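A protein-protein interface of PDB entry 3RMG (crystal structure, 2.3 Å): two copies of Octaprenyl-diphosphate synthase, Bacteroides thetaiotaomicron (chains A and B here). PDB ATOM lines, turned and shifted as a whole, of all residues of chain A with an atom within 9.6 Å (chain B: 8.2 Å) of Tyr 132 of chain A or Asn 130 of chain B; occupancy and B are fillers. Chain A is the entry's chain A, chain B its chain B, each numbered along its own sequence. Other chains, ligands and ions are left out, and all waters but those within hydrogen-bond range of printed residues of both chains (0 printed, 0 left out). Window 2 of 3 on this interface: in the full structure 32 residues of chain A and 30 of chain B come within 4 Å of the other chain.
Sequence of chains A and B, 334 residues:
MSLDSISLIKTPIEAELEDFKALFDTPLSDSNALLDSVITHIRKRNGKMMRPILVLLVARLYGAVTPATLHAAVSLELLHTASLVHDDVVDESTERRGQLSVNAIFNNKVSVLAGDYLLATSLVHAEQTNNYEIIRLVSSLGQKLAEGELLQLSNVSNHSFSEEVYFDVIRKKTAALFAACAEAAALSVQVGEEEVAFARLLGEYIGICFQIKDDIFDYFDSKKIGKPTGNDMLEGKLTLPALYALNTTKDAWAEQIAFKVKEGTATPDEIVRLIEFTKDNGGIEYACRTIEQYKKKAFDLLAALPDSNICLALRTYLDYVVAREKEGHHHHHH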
ATOM      1  N   ALA A  68      -0.884  13.997   9.886  1.00  0.00           N
ATOM      2  CA  ALA A  68      -1.674  12.755   9.918  1.00  0.00           C
ATOM      3  C   ALA A  68      -1.384  11.909  11.166  1.00  0.00           C
ATOM      4  O   ALA A  68      -2.290  11.291  11.724  1.00  0.00           O
ATOM      5  CB  ALA A  68      -1.440  11.926   8.642  1.00  0.00           C
ATOM      6  N   ALA A 126      -9.881  11.270  12.494  1.00  0.00           N
ATOM      7  CA  ALA A 126      -9.449  10.212  11.593  1.00  0.00           C
ATOM      8  C   ALA A 126      -9.521  10.682  10.137  1.00  0.00           C
ATOM      9  O   ALA A 126      -8.634  10.402   9.333  1.00  0.00           O
ATOM     10  CB  ALA A 126     -10.279   8.957  11.809  1.00  0.00           C
ATOM     11  N   GLU A 127     -10.579  11.406   9.796  1.00  0.00           N
ATOM     12  CA  GLU A 127     -10.755  11.869   8.424  1.00  0.00           C
ATOM     13  C   GLU A 127      -9.715  12.944   8.091  1.00  0.00           C
ATOM     14  O   GLU A 127      -9.065  12.914   7.034  1.00  0.00           O
ATOM     15  CB  GLU A 127     -12.188  12.365   8.226  1.00  0.00           C
ATOM     16  CG  GLU A 127     -12.497  12.829   6.820  1.00  0.00           C
ATOM     17  CD  GLU A 127     -11.978  14.231   6.571  1.00  0.00           C
ATOM     18  OE1 GLU A 127     -12.064  15.072   7.517  1.00  0.00           O
ATOM     19  OE2 GLU A 127     -11.492  14.472   5.440  1.00  0.00           O
ATOM     20  N   GLN A 128      -9.511  13.867   9.021  1.00  0.00           N
ATOM     21  CA  GLN A 128      -8.428  14.849   8.877  1.00  0.00           C
ATOM     22  C   GLN A 128      -7.019  14.268   8.664  1.00  0.00           C
ATOM     23  O   GLN A 128      -6.110  15.020   8.284  1.00  0.00           O
ATOM     24  CB  GLN A 128      -8.409  15.815  10.052  1.00  0.00           C
ATOM     25  CG  GLN A 128      -9.629  16.726  10.142  1.00  0.00           C
ATOM     26  CD  GLN A 128      -9.485  17.728  11.260  1.00  0.00           C
ATOM     27  OE1 GLN A 128      -9.913  17.481  12.391  1.00  0.00           O
ATOM     28  NE2 GLN A 128      -8.840  18.858  10.964  1.00  0.00           N
ATOM     29  N   THR A 129      -6.821  12.958   8.891  1.00  0.00           N
ATOM     30  CA  THR A 129      -5.556  12.316   8.482  1.00  0.00           C
ATOM     31  C   THR A 129      -5.450  12.203   6.967  1.00  0.00           C
ATOM     32  O   THR A 129      -4.387  11.870   6.421  1.00  0.00           O
ATOM     33  CB  THR A 129      -5.386  10.861   9.013  1.00  0.00           C
ATOM     34  OG1 THR A 129      -6.207   9.964   8.247  1.00  0.00           O
ATOM     35  CG2 THR A 129      -5.717  10.750  10.498  1.00  0.00           C
ATOM     36  N   ASN A 130      -6.565  12.422   6.285  1.00  0.00           N
ATOM     37  CA  ASN A 130      -6.619  12.211   4.838  1.00  0.00           C
ATOM     38  C   ASN A 130      -6.061  10.856   4.426  1.00  0.00           C
ATOM     39  O   ASN A 130      -5.475  10.724   3.354  1.00  0.00           O
ATOM     40  CB  ASN A 130      -5.880  13.326   4.089  1.00  0.00           C
ATOM     41  CG  ASN A 130      -6.376  14.724   4.471  1.00  0.00           C
ATOM     42  OD1 ASN A 130      -7.582  14.993   4.491  1.00  0.00           O
ATOM     43  ND2 ASN A 130      -5.437  15.624   4.769  1.00  0.00           N
ATOM     44  N   ASN A 131      -6.244   9.845   5.270  1.00  0.00           N
ATOM     45  CA  ASN A 131      -5.740   8.509   4.960  1.00  0.00           C
ATOM     46  C   ASN A 131      -6.825   7.454   5.183  1.00  0.00           C
ATOM     47  O   ASN A 131      -7.342   7.310   6.291  1.00  0.00           O
ATOM     48  CB  ASN A 131      -4.463   8.216   5.767  1.00  0.00           C
ATOM     49  CG  ASN A 131      -3.838   6.870   5.431  1.00  0.00           C
ATOM     50  OD1 ASN A 131      -4.531   5.911   5.093  1.00  0.00           O
ATOM     51  ND2 ASN A 131      -2.517   6.794   5.535  1.00  0.00           N
ATOM     52  N   TYR A 132      -7.168   6.730   4.119  1.00  0.00           N
ATOM     53  CA  TYR A 132      -8.320   5.815   4.125  1.00  0.00           C
ATOM     54  C   TYR A 132      -8.136   4.663   5.091  1.00  0.00           C
ATOM     55  O   TYR A 132      -9.063   4.293   5.844  1.00  0.00           O
ATOM     56  CB  TYR A 132      -8.583   5.256   2.715  1.00  0.00           C
ATOM     57  CG  TYR A 132      -9.352   6.211   1.815  1.00  0.00           C
ATOM     58  CD1 TYR A 132     -10.667   6.564   2.105  1.00  0.00           C
ATOM     59  CD2 TYR A 132      -8.765   6.754   0.680  1.00  0.00           C
ATOM     60  CE1 TYR A 132     -11.371   7.438   1.300  1.00  0.00           C
ATOM     61  CE2 TYR A 132      -9.465   7.630  -0.142  1.00  0.00           C
ATOM     62  CZ  TYR A 132     -10.766   7.968   0.174  1.00  0.00           C
ATOM     63  OH  TYR A 132     -11.462   8.838  -0.639  1.00  0.00           O
ATOM     64  N   GLU A 133      -6.941   4.087   5.052  1.00  0.00           N
ATOM     65  CA  GLU A 133      -6.604   2.949   5.886  1.00  0.00           C
ATOM     66  C   GLU A 133      -6.756   3.329   7.343  1.00  0.00           C
ATOM     67  O   GLU A 133      -7.264   2.553   8.163  1.00  0.00           O
ATOM     68  CB  GLU A 133      -5.190   2.504   5.591  1.00  0.00           C
ATOM     69  CG  GLU A 133      -4.961   2.294   4.095  1.00  0.00           C
ATOM     70  CD  GLU A 133      -3.888   1.275   3.805  1.00  0.00           C
ATOM     71  OE1 GLU A 133      -3.958   0.157   4.366  1.00  0.00           O
ATOM     72  OE2 GLU A 133      -2.976   1.590   3.009  1.00  0.00           O
ATOM     73  N   ILE A 134      -6.348   4.544   7.661  1.00  0.00           N
ATOM     74  CA  ILE A 134      -6.413   4.990   9.033  1.00  0.00           C
ATOM     75  C   ILE A 134      -7.869   5.182   9.384  1.00  0.00           C
ATOM     76  O   ILE A 134      -8.306   4.863  10.490  1.00  0.00           O
ATOM     77  CB  ILE A 134      -5.623   6.286   9.243  1.00  0.00           C
ATOM     78  CG1 ILE A 134      -4.120   5.984   9.189  1.00  0.00           C
ATOM     79  CG2 ILE A 134      -6.017   6.913  10.543  1.00  0.00           C
ATOM     80  CD1 ILE A 134      -3.227   7.242   9.196  1.00  0.00           C
ATOM     81  N   ILE A 135      -8.632   5.700   8.432  1.00  0.00           N
ATOM     82  CA  ILE A 135     -10.065   5.830   8.625  1.00  0.00           C
ATOM     83  C   ILE A 135     -10.683   4.442   8.808  1.00  0.00           C
ATOM     84  O   ILE A 135     -11.463   4.203   9.721  1.00  0.00           O
ATOM     85  CB  ILE A 135     -10.714   6.595   7.457  1.00  0.00           C
ATOM     86  CG1 ILE A 135     -10.195   8.047   7.447  1.00  0.00           C
ATOM     87  CG2 ILE A 135     -12.232   6.573   7.592  1.00  0.00           C
ATOM     88  CD1 ILE A 135     -10.625   8.883   6.259  1.00  0.00           C
ATOM     89  N   ARG A 136     -10.305   3.518   7.937  1.00  0.00           N
ATOM     90  CA  ARG A 136     -10.744   2.145   8.076  1.00  0.00           C
ATOM     91  C   ARG A 136     -10.354   1.579   9.444  1.00  0.00           C
ATOM     92  O   ARG A 136     -11.168   0.941  10.114  1.00  0.00           O
ATOM     93  CB  ARG A 136     -10.150   1.292   6.955  1.00  0.00           C
ATOM     94  CG  ARG A 136     -10.979   0.076   6.600  1.00  0.00           C
ATOM     95  CD  ARG A 136     -11.038  -0.091   5.090  1.00  0.00           C
ATOM     96  NE  ARG A 136      -9.769   0.268   4.458  1.00  0.00           N
ATOM     97  CZ  ARG A 136      -9.644   0.698   3.205  1.00  0.00           C
ATOM     98  NH1 ARG A 136     -10.713   0.825   2.431  1.00  0.00           N
ATOM     99  NH2 ARG A 136      -8.447   1.000   2.721  1.00  0.00           N
ATOM    100  N   LEU A 137      -9.114   1.818   9.864  1.00  0.00           N
ATOM    101  CA  LEU A 137      -8.619   1.250  11.113  1.00  0.00           C
ATOM    102  C   LEU A 137      -9.415   1.778  12.304  1.00  0.00           C
ATOM    103  O   LEU A 137      -9.828   1.028  13.184  1.00  0.00           O
ATOM    104  CB  LEU A 137      -7.116   1.532  11.278  1.00  0.00           C
ATOM    105  CG  LEU A 137      -6.468   1.328  12.655  1.00  0.00           C
ATOM    106  CD1 LEU A 137      -4.963   1.229  12.558  1.00  0.00           C
ATOM    107  CD2 LEU A 137      -6.834   2.470  13.579  1.00  0.00           C
ATOM    108  N   VAL A 138      -9.632   3.081  12.344  1.00  0.00           N
ATOM    109  CA  VAL A 138     -10.301   3.645  13.498  1.00  0.00           C
ATOM    110  C   VAL A 138     -11.756   3.222  13.518  1.00  0.00           C
ATOM    111  O   VAL A 138     -12.312   2.897  14.579  1.00  0.00           O
ATOM    112  CB  VAL A 138     -10.257   5.169  13.490  1.00  0.00           C
ATOM    113  CG1 VAL A 138     -11.140   5.697  14.610  1.00  0.00           C
ATOM    114  CG2 VAL A 138      -8.827   5.649  13.650  1.00  0.00           C
ATOM    115  N   SER A 139     -12.399   3.238  12.352  1.00  0.00           N
ATOM    116  CA  SER A 139     -13.814   2.902  12.356  1.00  0.00           C
ATOM    117  C   SER A 139     -13.998   1.427  12.717  1.00  0.00           C
ATOM    118  O   SER A 139     -14.782   1.100  13.608  1.00  0.00           O
ATOM    119  CB  SER A 139     -14.526   3.305  11.045  1.00  0.00           C
ATOM    120  OG  SER A 139     -14.075   2.566   9.915  1.00  0.00           O
ATOM    121  N   SER A 140     -13.256   0.530  12.069  1.00  0.00           N
ATOM    122  CA  SER A 140     -13.445  -0.887  12.384  1.00  0.00           C
ATOM    123  C   SER A 140     -13.118  -1.177  13.842  1.00  0.00           C
ATOM    124  O   SER A 140     -13.772  -1.997  14.477  1.00  0.00           O
ATOM    125  CB  SER A 140     -12.649  -1.795  11.448  1.00  0.00           C
ATOM    126  OG  SER A 140     -11.269  -1.625  11.651  1.00  0.00           O
ATOM    127  N   LEU A 187       1.043   3.596   9.234  1.00  0.00           N
ATOM    128  CA  LEU A 187       0.271   4.090   8.105  1.00  0.00           C
ATOM    129  C   LEU A 187       0.448   5.604   7.899  1.00  0.00           C
ATOM    130  O   LEU A 187       0.516   6.079   6.760  1.00  0.00           O
ATOM    131  CB  LEU A 187      -1.210   3.765   8.282  1.00  0.00           C
ATOM    132  CG  LEU A 187      -1.578   2.282   8.247  1.00  0.00           C
ATOM    133  CD1 LEU A 187      -2.959   2.069   8.884  1.00  0.00           C
ATOM    134  CD2 LEU A 187      -1.502   1.718   6.841  1.00  0.00           C
ATOM    135  N   SER A 188       0.542   6.355   8.994  1.00  0.00           N
ATOM    136  CA  SER A 188       0.588   7.821   8.917  1.00  0.00           C
ATOM    137  C   SER A 188       1.847   8.354   8.249  1.00  0.00           C
ATOM    138  O   SER A 188       1.854   9.484   7.775  1.00  0.00           O
ATOM    139  CB  SER A 188       0.444   8.449  10.306  1.00  0.00           C
ATOM    140  OG  SER A 188       1.662   8.383  11.034  1.00  0.00           O
ATOM    141  N   GLN A 190       3.292   6.342   5.966  1.00  0.00           N
ATOM    142  CA  GLN A 190       3.203   5.717   4.651  1.00  0.00           C
ATOM    143  C   GLN A 190       4.291   4.698   4.345  1.00  0.00           C
ATOM    144  O   GLN A 190       4.849   4.709   3.251  1.00  0.00           O
ATOM    145  CB  GLN A 190       3.212   6.793   3.567  1.00  0.00           C
ATOM    146  CG  GLN A 190       2.127   7.829   3.747  1.00  0.00           C
ATOM    147  CD  GLN A 190       2.036   8.770   2.577  1.00  0.00           C
ATOM    148  OE1 GLN A 190       3.053   9.173   2.011  1.00  0.00           O
ATOM    149  NE2 GLN A 190       0.816   9.129   2.200  1.00  0.00           N
ATOM    150  N   PRO B  67     -22.418   2.623  -5.738  1.00  0.00           N
ATOM    151  CA  PRO B  67     -22.264   1.943  -4.449  1.00  0.00           C
ATOM    152  C   PRO B  67     -21.960   2.973  -3.366  1.00  0.00           C
ATOM    153  O   PRO B  67     -22.435   2.842  -2.227  1.00  0.00           O
ATOM    154  CB  PRO B  67     -21.065   1.015  -4.677  1.00  0.00           C
ATOM    155  CG  PRO B  67     -21.032   0.798  -6.186  1.00  0.00           C
ATOM    156  CD  PRO B  67     -21.459   2.137  -6.748  1.00  0.00           C
ATOM    157  N   ALA B  68     -21.205   4.011  -3.728  1.00  0.00           N
ATOM    158  CA  ALA B  68     -21.000   5.131  -2.822  1.00  0.00           C
ATOM    159  C   ALA B  68     -22.352   5.676  -2.349  1.00  0.00           C
ATOM    160  O   ALA B  68     -22.548   5.918  -1.156  1.00  0.00           O
ATOM    161  CB  ALA B  68     -20.180   6.222  -3.494  1.00  0.00           C
ATOM    162  N   HIS B  71     -23.865   3.228   0.271  1.00  0.00           N
ATOM    163  CA  HIS B  71     -23.156   3.246   1.543  1.00  0.00           C
ATOM    164  C   HIS B  71     -23.473   4.528   2.300  1.00  0.00           C
ATOM    165  O   HIS B  71     -23.625   4.520   3.522  1.00  0.00           O
ATOM    166  CB  HIS B  71     -21.644   3.087   1.333  1.00  0.00           C
ATOM    167  CG  HIS B  71     -21.224   1.672   1.086  1.00  0.00           C
ATOM    168  ND1 HIS B  71     -21.418   0.669   2.012  1.00  0.00           N
ATOM    169  CD2 HIS B  71     -20.627   1.091   0.018  1.00  0.00           C
ATOM    170  CE1 HIS B  71     -20.961  -0.471   1.522  1.00  0.00           C
ATOM    171  NE2 HIS B  71     -20.472  -0.241   0.316  1.00  0.00           N
ATOM    172  N   ALA B  72     -23.581   5.632   1.568  1.00  0.00           N
ATOM    173  CA  ALA B  72     -23.967   6.892   2.182  1.00  0.00           C
ATOM    174  C   ALA B  72     -25.331   6.780   2.870  1.00  0.00           C
ATOM    175  O   ALA B  72     -25.492   7.214   4.010  1.00  0.00           O
ATOM    176  CB  ALA B  72     -23.971   8.005   1.147  1.00  0.00           C
ATOM    177  N   VAL B 124     -18.291   3.112   9.462  1.00  0.00           N
ATOM    178  CA  VAL B 124     -17.796   2.055   8.572  1.00  0.00           C
ATOM    179  C   VAL B 124     -18.418   2.233   7.188  1.00  0.00           C
ATOM    180  O   VAL B 124     -17.729   2.272   6.171  1.00  0.00           O
ATOM    181  CB  VAL B 124     -18.086   0.639   9.146  1.00  0.00           C
ATOM    182  CG1 VAL B 124     -17.635  -0.463   8.177  1.00  0.00           C
ATOM    183  CG2 VAL B 124     -17.419   0.482  10.514  1.00  0.00           C
ATOM    184  N   HIS B 125     -19.728   2.398   7.137  1.00  0.00           N
ATOM    185  CA  HIS B 125     -20.345   2.613   5.827  1.00  0.00           C
ATOM    186  C   HIS B 125     -19.881   3.915   5.165  1.00  0.00           C
ATOM    187  O   HIS B 125     -19.687   3.966   3.947  1.00  0.00           O
ATOM    188  CB  HIS B 125     -21.863   2.471   5.913  1.00  0.00           C
ATOM    189  CG  HIS B 125     -22.308   1.045   5.931  1.00  0.00           C
ATOM    190  ND1 HIS B 125     -22.293   0.254   4.801  1.00  0.00           N
ATOM    191  CD2 HIS B 125     -22.742   0.254   6.940  1.00  0.00           C
ATOM    192  CE1 HIS B 125     -22.712  -0.961   5.114  1.00  0.00           C
ATOM    193  NE2 HIS B 125     -22.996  -0.986   6.405  1.00  0.00           N
ATOM    194  N   ALA B 126     -19.661   4.957   5.963  1.00  0.00           N
ATOM    195  CA  ALA B 126     -19.151   6.218   5.411  1.00  0.00           C
ATOM    196  C   ALA B 126     -17.782   6.046   4.754  1.00  0.00           C
ATOM    197  O   ALA B 126     -17.500   6.605   3.678  1.00  0.00           O
ATOM    198  CB  ALA B 126     -19.093   7.282   6.479  1.00  0.00           C
ATOM    199  N   GLU B 127     -16.918   5.277   5.403  1.00  0.00           N
ATOM    200  CA  GLU B 127     -15.607   5.003   4.825  1.00  0.00           C
ATOM    201  C   GLU B 127     -15.732   4.134   3.560  1.00  0.00           C
ATOM    202  O   GLU B 127     -15.061   4.372   2.553  1.00  0.00           O
ATOM    203  CB  GLU B 127     -14.696   4.352   5.866  1.00  0.00           C
ATOM    204  CG  GLU B 127     -13.277   4.159   5.392  1.00  0.00           C
ATOM    205  CD  GLU B 127     -13.138   2.934   4.525  1.00  0.00           C
ATOM    206  OE1 GLU B 127     -13.800   1.909   4.847  1.00  0.00           O
ATOM    207  OE2 GLU B 127     -12.372   3.014   3.534  1.00  0.00           O
ATOM    208  N   GLN B 128     -16.611   3.140   3.603  1.00  0.00           N
ATOM    209  CA  GLN B 128     -16.852   2.321   2.418  1.00  0.00           C
ATOM    210  C   GLN B 128     -17.359   3.086   1.190  1.00  0.00           C
ATOM    211  O   GLN B 128     -17.417   2.507   0.106  1.00  0.00           O
ATOM    212  CB  GLN B 128     -17.814   1.184   2.747  1.00  0.00           C
ATOM    213  CG  GLN B 128     -17.176   0.072   3.538  1.00  0.00           C
ATOM    214  CD  GLN B 128     -18.192  -0.902   4.081  1.00  0.00           C
ATOM    215  OE1 GLN B 128     -18.285  -2.038   3.621  1.00  0.00           O
ATOM    216  NE2 GLN B 128     -18.972  -0.458   5.058  1.00  0.00           N
ATOM    217  N   THR B 129     -17.750   4.359   1.340  1.00  0.00           N
ATOM    218  CA  THR B 129     -18.100   5.179   0.155  1.00  0.00           C
ATOM    219  C   THR B 129     -16.867   5.553  -0.647  1.00  0.00           C
ATOM    220  O   THR B 129     -16.980   6.110  -1.741  1.00  0.00           O
ATOM    221  CB  THR B 129     -18.754   6.540   0.515  1.00  0.00           C
ATOM    222  OG1 THR B 129     -17.806   7.350   1.218  1.00  0.00           O
ATOM    223  CG2 THR B 129     -20.006   6.366   1.362  1.00  0.00           C
ATOM    224  N   ASN B 130     -15.688   5.281  -0.088  1.00  0.00           N
ATOM    225  CA  ASN B 130     -14.438   5.670  -0.725  1.00  0.00           C
ATOM    226  C   ASN B 130     -14.449   7.129  -1.189  1.00  0.00           C
ATOM    227  O   ASN B 130     -13.980   7.427  -2.279  1.00  0.00           O
ATOM    228  CB  ASN B 130     -14.141   4.747  -1.919  1.00  0.00           C
ATOM    229  CG  ASN B 130     -14.136   3.270  -1.537  1.00  0.00           C
ATOM    230  OD1 ASN B 130     -13.669   2.892  -0.464  1.00  0.00           O
ATOM    231  ND2 ASN B 130     -14.653   2.429  -2.427  1.00  0.00           N
ATOM    232  N   ASN B 131     -14.986   8.027  -0.369  1.00  0.00           N
ATOM    233  CA  ASN B 131     -15.104   9.426  -0.753  1.00  0.00           C
ATOM    234  C   ASN B 131     -14.942  10.369   0.448  1.00  0.00           C
ATOM    235  O   ASN B 131     -15.772  10.383   1.367  1.00  0.00           O
ATOM    236  CB  ASN B 131     -16.453   9.633  -1.439  1.00  0.00           C
ATOM    237  CG  ASN B 131     -16.794  11.082  -1.633  1.00  0.00           C
ATOM    238  OD1 ASN B 131     -16.521  11.921  -0.775  1.00  0.00           O
ATOM    239  ND2 ASN B 131     -17.432  11.386  -2.750  1.00  0.00           N
ATOM    240  N   TYR B 132     -13.873  11.157   0.446  1.00  0.00           N
ATOM    241  CA  TYR B 132     -13.503  11.912   1.641  1.00  0.00           C
ATOM    242  C   TYR B 132     -14.578  12.893   2.077  1.00  0.00           C
ATOM    243  O   TYR B 132     -14.875  13.024   3.274  1.00  0.00           O
ATOM    244  CB  TYR B 132     -12.162  12.639   1.445  1.00  0.00           C
ATOM    245  CG  TYR B 132     -10.943  11.727   1.535  1.00  0.00           C
ATOM    246  CD1 TYR B 132     -10.500  11.236   2.765  1.00  0.00           C
ATOM    247  CD2 TYR B 132     -10.228  11.366   0.391  1.00  0.00           C
ATOM    248  CE1 TYR B 132      -9.390  10.412   2.853  1.00  0.00           C
ATOM    249  CE2 TYR B 132      -9.110  10.540   0.468  1.00  0.00           C
ATOM    250  CZ  TYR B 132      -8.698  10.061   1.701  1.00  0.00           C
ATOM    251  OH  TYR B 132      -7.590   9.240   1.789  1.00  0.00           O
ATOM    252  N   GLU B 133     -15.166  13.595   1.116  1.00  0.00           N
ATOM    253  CA  GLU B 133     -16.153  14.612   1.455  1.00  0.00           C
ATOM    254  C   GLU B 133     -17.362  14.024   2.179  1.00  0.00           C
ATOM    255  O   GLU B 133     -17.904  14.634   3.096  1.00  0.00           O
ATOM    256  CB  GLU B 133     -16.569  15.355   0.206  1.00  0.00           C
ATOM    257  CG  GLU B 133     -15.370  15.732  -0.640  1.00  0.00           C
ATOM    258  CD  GLU B 133     -15.753  16.586  -1.815  1.00  0.00           C
ATOM    259  OE1 GLU B 133     -16.145  17.757  -1.594  1.00  0.00           O
ATOM    260  OE2 GLU B 133     -15.655  16.077  -2.956  1.00  0.00           O
ATOM    261  N   ILE B 134     -17.774  12.828   1.777  1.00  0.00           N
ATOM    262  CA  ILE B 134     -18.866  12.164   2.460  1.00  0.00           C
ATOM    263  C   ILE B 134     -18.474  11.778   3.898  1.00  0.00           C
ATOM    264  O   ILE B 134     -19.238  12.020   4.832  1.00  0.00           O
ATOM    265  CB  ILE B 134     -19.346  10.952   1.670  1.00  0.00           C
ATOM    266  CG1 ILE B 134     -19.945  11.418   0.333  1.00  0.00           C
ATOM    267  CG2 ILE B 134     -20.337  10.137   2.483  1.00  0.00           C
ATOM    268  CD1 ILE B 134     -20.452  10.275  -0.542  1.00  0.00           C
ATOM    269  N   ILE B 135     -17.288  11.192   4.075  1.00  0.00           N
ATOM    270  CA  ILE B 135     -16.771  10.898   5.411  1.00  0.00           C
ATOM    271  C   ILE B 135     -16.712  12.158   6.268  1.00  0.00           C
ATOM    272  O   ILE B 135     -17.056  12.138   7.442  1.00  0.00           O
ATOM    273  CB  ILE B 135     -15.368  10.258   5.359  1.00  0.00           C
ATOM    274  CG1 ILE B 135     -15.447   8.891   4.667  1.00  0.00           C
ATOM    275  CG2 ILE B 135     -14.801  10.119   6.772  1.00  0.00           C
ATOM    276  CD1 ILE B 135     -14.118   8.346   4.217  1.00  0.00           C
ATOM    277  N   ARG B 136     -16.298  13.259   5.664  1.00  0.00           N
ATOM    278  CA  ARG B 136     -16.299  14.548   6.346  1.00  0.00           C
ATOM    279  C   ARG B 136     -17.726  14.941   6.712  1.00  0.00           C
ATOM    280  O   ARG B 136     -18.001  15.436   7.801  1.00  0.00           O
ATOM    281  CB  ARG B 136     -15.671  15.602   5.441  1.00  0.00           C
ATOM    282  CG  ARG B 136     -15.117  16.830   6.154  1.00  0.00           C
ATOM    283  CD  ARG B 136     -14.187  17.589   5.202  1.00  0.00           C
ATOM    284  NE  ARG B 136     -13.289  16.647   4.550  1.00  0.00           N
ATOM    285  CZ  ARG B 136     -12.781  16.800   3.331  1.00  0.00           C
ATOM    286  NH1 ARG B 136     -13.084  17.870   2.610  1.00  0.00           N
ATOM    287  NH2 ARG B 136     -11.974  15.871   2.831  1.00  0.00           N
ATOM    288  N   GLN B 190     -20.703  12.544  -7.659  1.00  0.00           N
ATOM    289  CA  GLN B 190     -19.624  13.431  -8.045  1.00  0.00           C
ATOM    290  C   GLN B 190     -20.022  14.594  -8.945  1.00  0.00           C
ATOM    291  O   GLN B 190     -19.331  14.864  -9.928  1.00  0.00           O
ATOM    292  CB  GLN B 190     -18.487  12.648  -8.718  1.00  0.00           C
ATOM    293  CG  GLN B 190     -18.363  11.224  -8.254  1.00  0.00           C
ATOM    294  CD  GLN B 190     -16.957  10.697  -8.363  1.00  0.00           C
ATOM    295  OE1 GLN B 190     -16.722   9.651  -8.969  1.00  0.00           O
ATOM    296  NE2 GLN B 190     -16.005  11.418  -7.774  1.00  0.00           N
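Of the printed residues of chain B, Glu 127 of chain A touches Ile 135 and Arg 136. Of the printed residues of chain B, Tyr 132 of chain A touches Asn 130, Asn 131 and Tyr 132. Printed residues of chain A within 4 Å of Val 124 of chain B: Ser 139 (3.99 Å). Ala 126 of chain B touches none of the printed residues of chain A. Printed residues of chain A within 4 Å of Asn 130 of chain B: Tyr 132 (3.3 Å). Asn 131 of chain B touches one residue of chain A. Printed residues of chain A within 4 Å of Ile 135 of chain B: Glu 127 (3.6 Å). The nearest printed residue of chain A that does not touch Asn 130 of chain B is Arg 136 of chain A (4.6 Å). The nearest printed residue of chain B that does not touch Ile 135 of chain A is Ile 135 of chain B (4.1 Å).
O of Val 124 of chain B sits at hydrogen-bond distance from NE2 of Gln 128 of chain B (3.2 Å). O of Arg 136 of chain A lies within hydrogen-bond range of OG of Ser 140 of chain A (3.0 Å). OG of Ser 139 of chain A is in hydrogen-bond range of O of Arg 136 of chain A, at 3.3 Å. OG1 of Thr 129 of chain B sits close to N of Asn 131 of chain B (3.3 Å). N of Ile 134 of chain B lies within hydrogen-bond range of OD1 of Asn 131 of chain B (3.0 Å).
OH of Tyr 132 of chain B sits close to N of Tyr 132 of chain A, 3.5 Å away. The side-chain carboxylate (OE2) of Glu 127 of chain A is in salt-bridge range of the guanidinium group (NE) of Arg 136 of chain B (3.0 Å). The backbone carbonyl oxygen of Asn 130 of chain B sits at hydrogen-bond distance from the side-chain hydroxyl of Tyr 132 of chain A (3.3 Å). OE2 of Glu 127 of chain B is in salt-bridge range of NH1 of Arg 136 of chain A, 3.0 Å away. The backbone carbonyl oxygen (O) of Asn 130 of chain A lies within hydrogen-bond range of the side-chain hydroxyl (OH) of Tyr 132 of chain B, at 3.0 Å.
Of the 19 printed residues of chain A, 7 touch a printed residue of chain B. Of the 18 printed residues of chain B, 7 touch a printed residue of chain A. Printed residues of chain B that touch a printed residue of chain A: Val 124, Glu 127, Asn 130, Asn 131, Tyr 132, Ile 135 and Arg 136. Among the printed residues, 11 pairs touch across the chains. Among the printed residues, Asp or Glu carboxylates within 4 Å of a Lys or Arg side-chain nitrogen of the other chain: Glu 127 of chain A with Arg 136 of chain B (3.0 Å) and Arg 136 of chain A with Glu 127 of chain B (3.0 Å).
Asn 130 of chain A touches Tyr 132 of chain B, and with the chains exchanged Tyr 132 of chain A touches Asn 130 of chain B. Asn 131 of chain A touches Tyr 132 of chain B, and with the chains exchanged Tyr 132 of chain A touches Asn 131 of chain B. Ile 135 of chain A touches Tyr 132 of chain B, but with the chains exchanged Tyr 132 of chain A does not touch Ile 135 of chain B (4.1 Å). Positions printed for both chains: 68, 126, 127, 128, 129, 130, 131, 132, 133, 134, 135, 136 and 190.
Glu 127 of chain A touches Ile 135 of chain B. CA of Asn 131 of chain A touches OH of Tyr 132 of chain B, at 3.7 Å. OH of Tyr 132 of chain A touches N of Asn 131 of chain B (3.6 Å). CG2 of Ile 135 of chain A touches CG of Glu 127 of chain B (3.4 Å). Ile 135 of chain A touches Tyr 132 of chain B. Val 124 of chain B touches Ser 139 of chain A (CG2 to OG, 3.99 Å).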
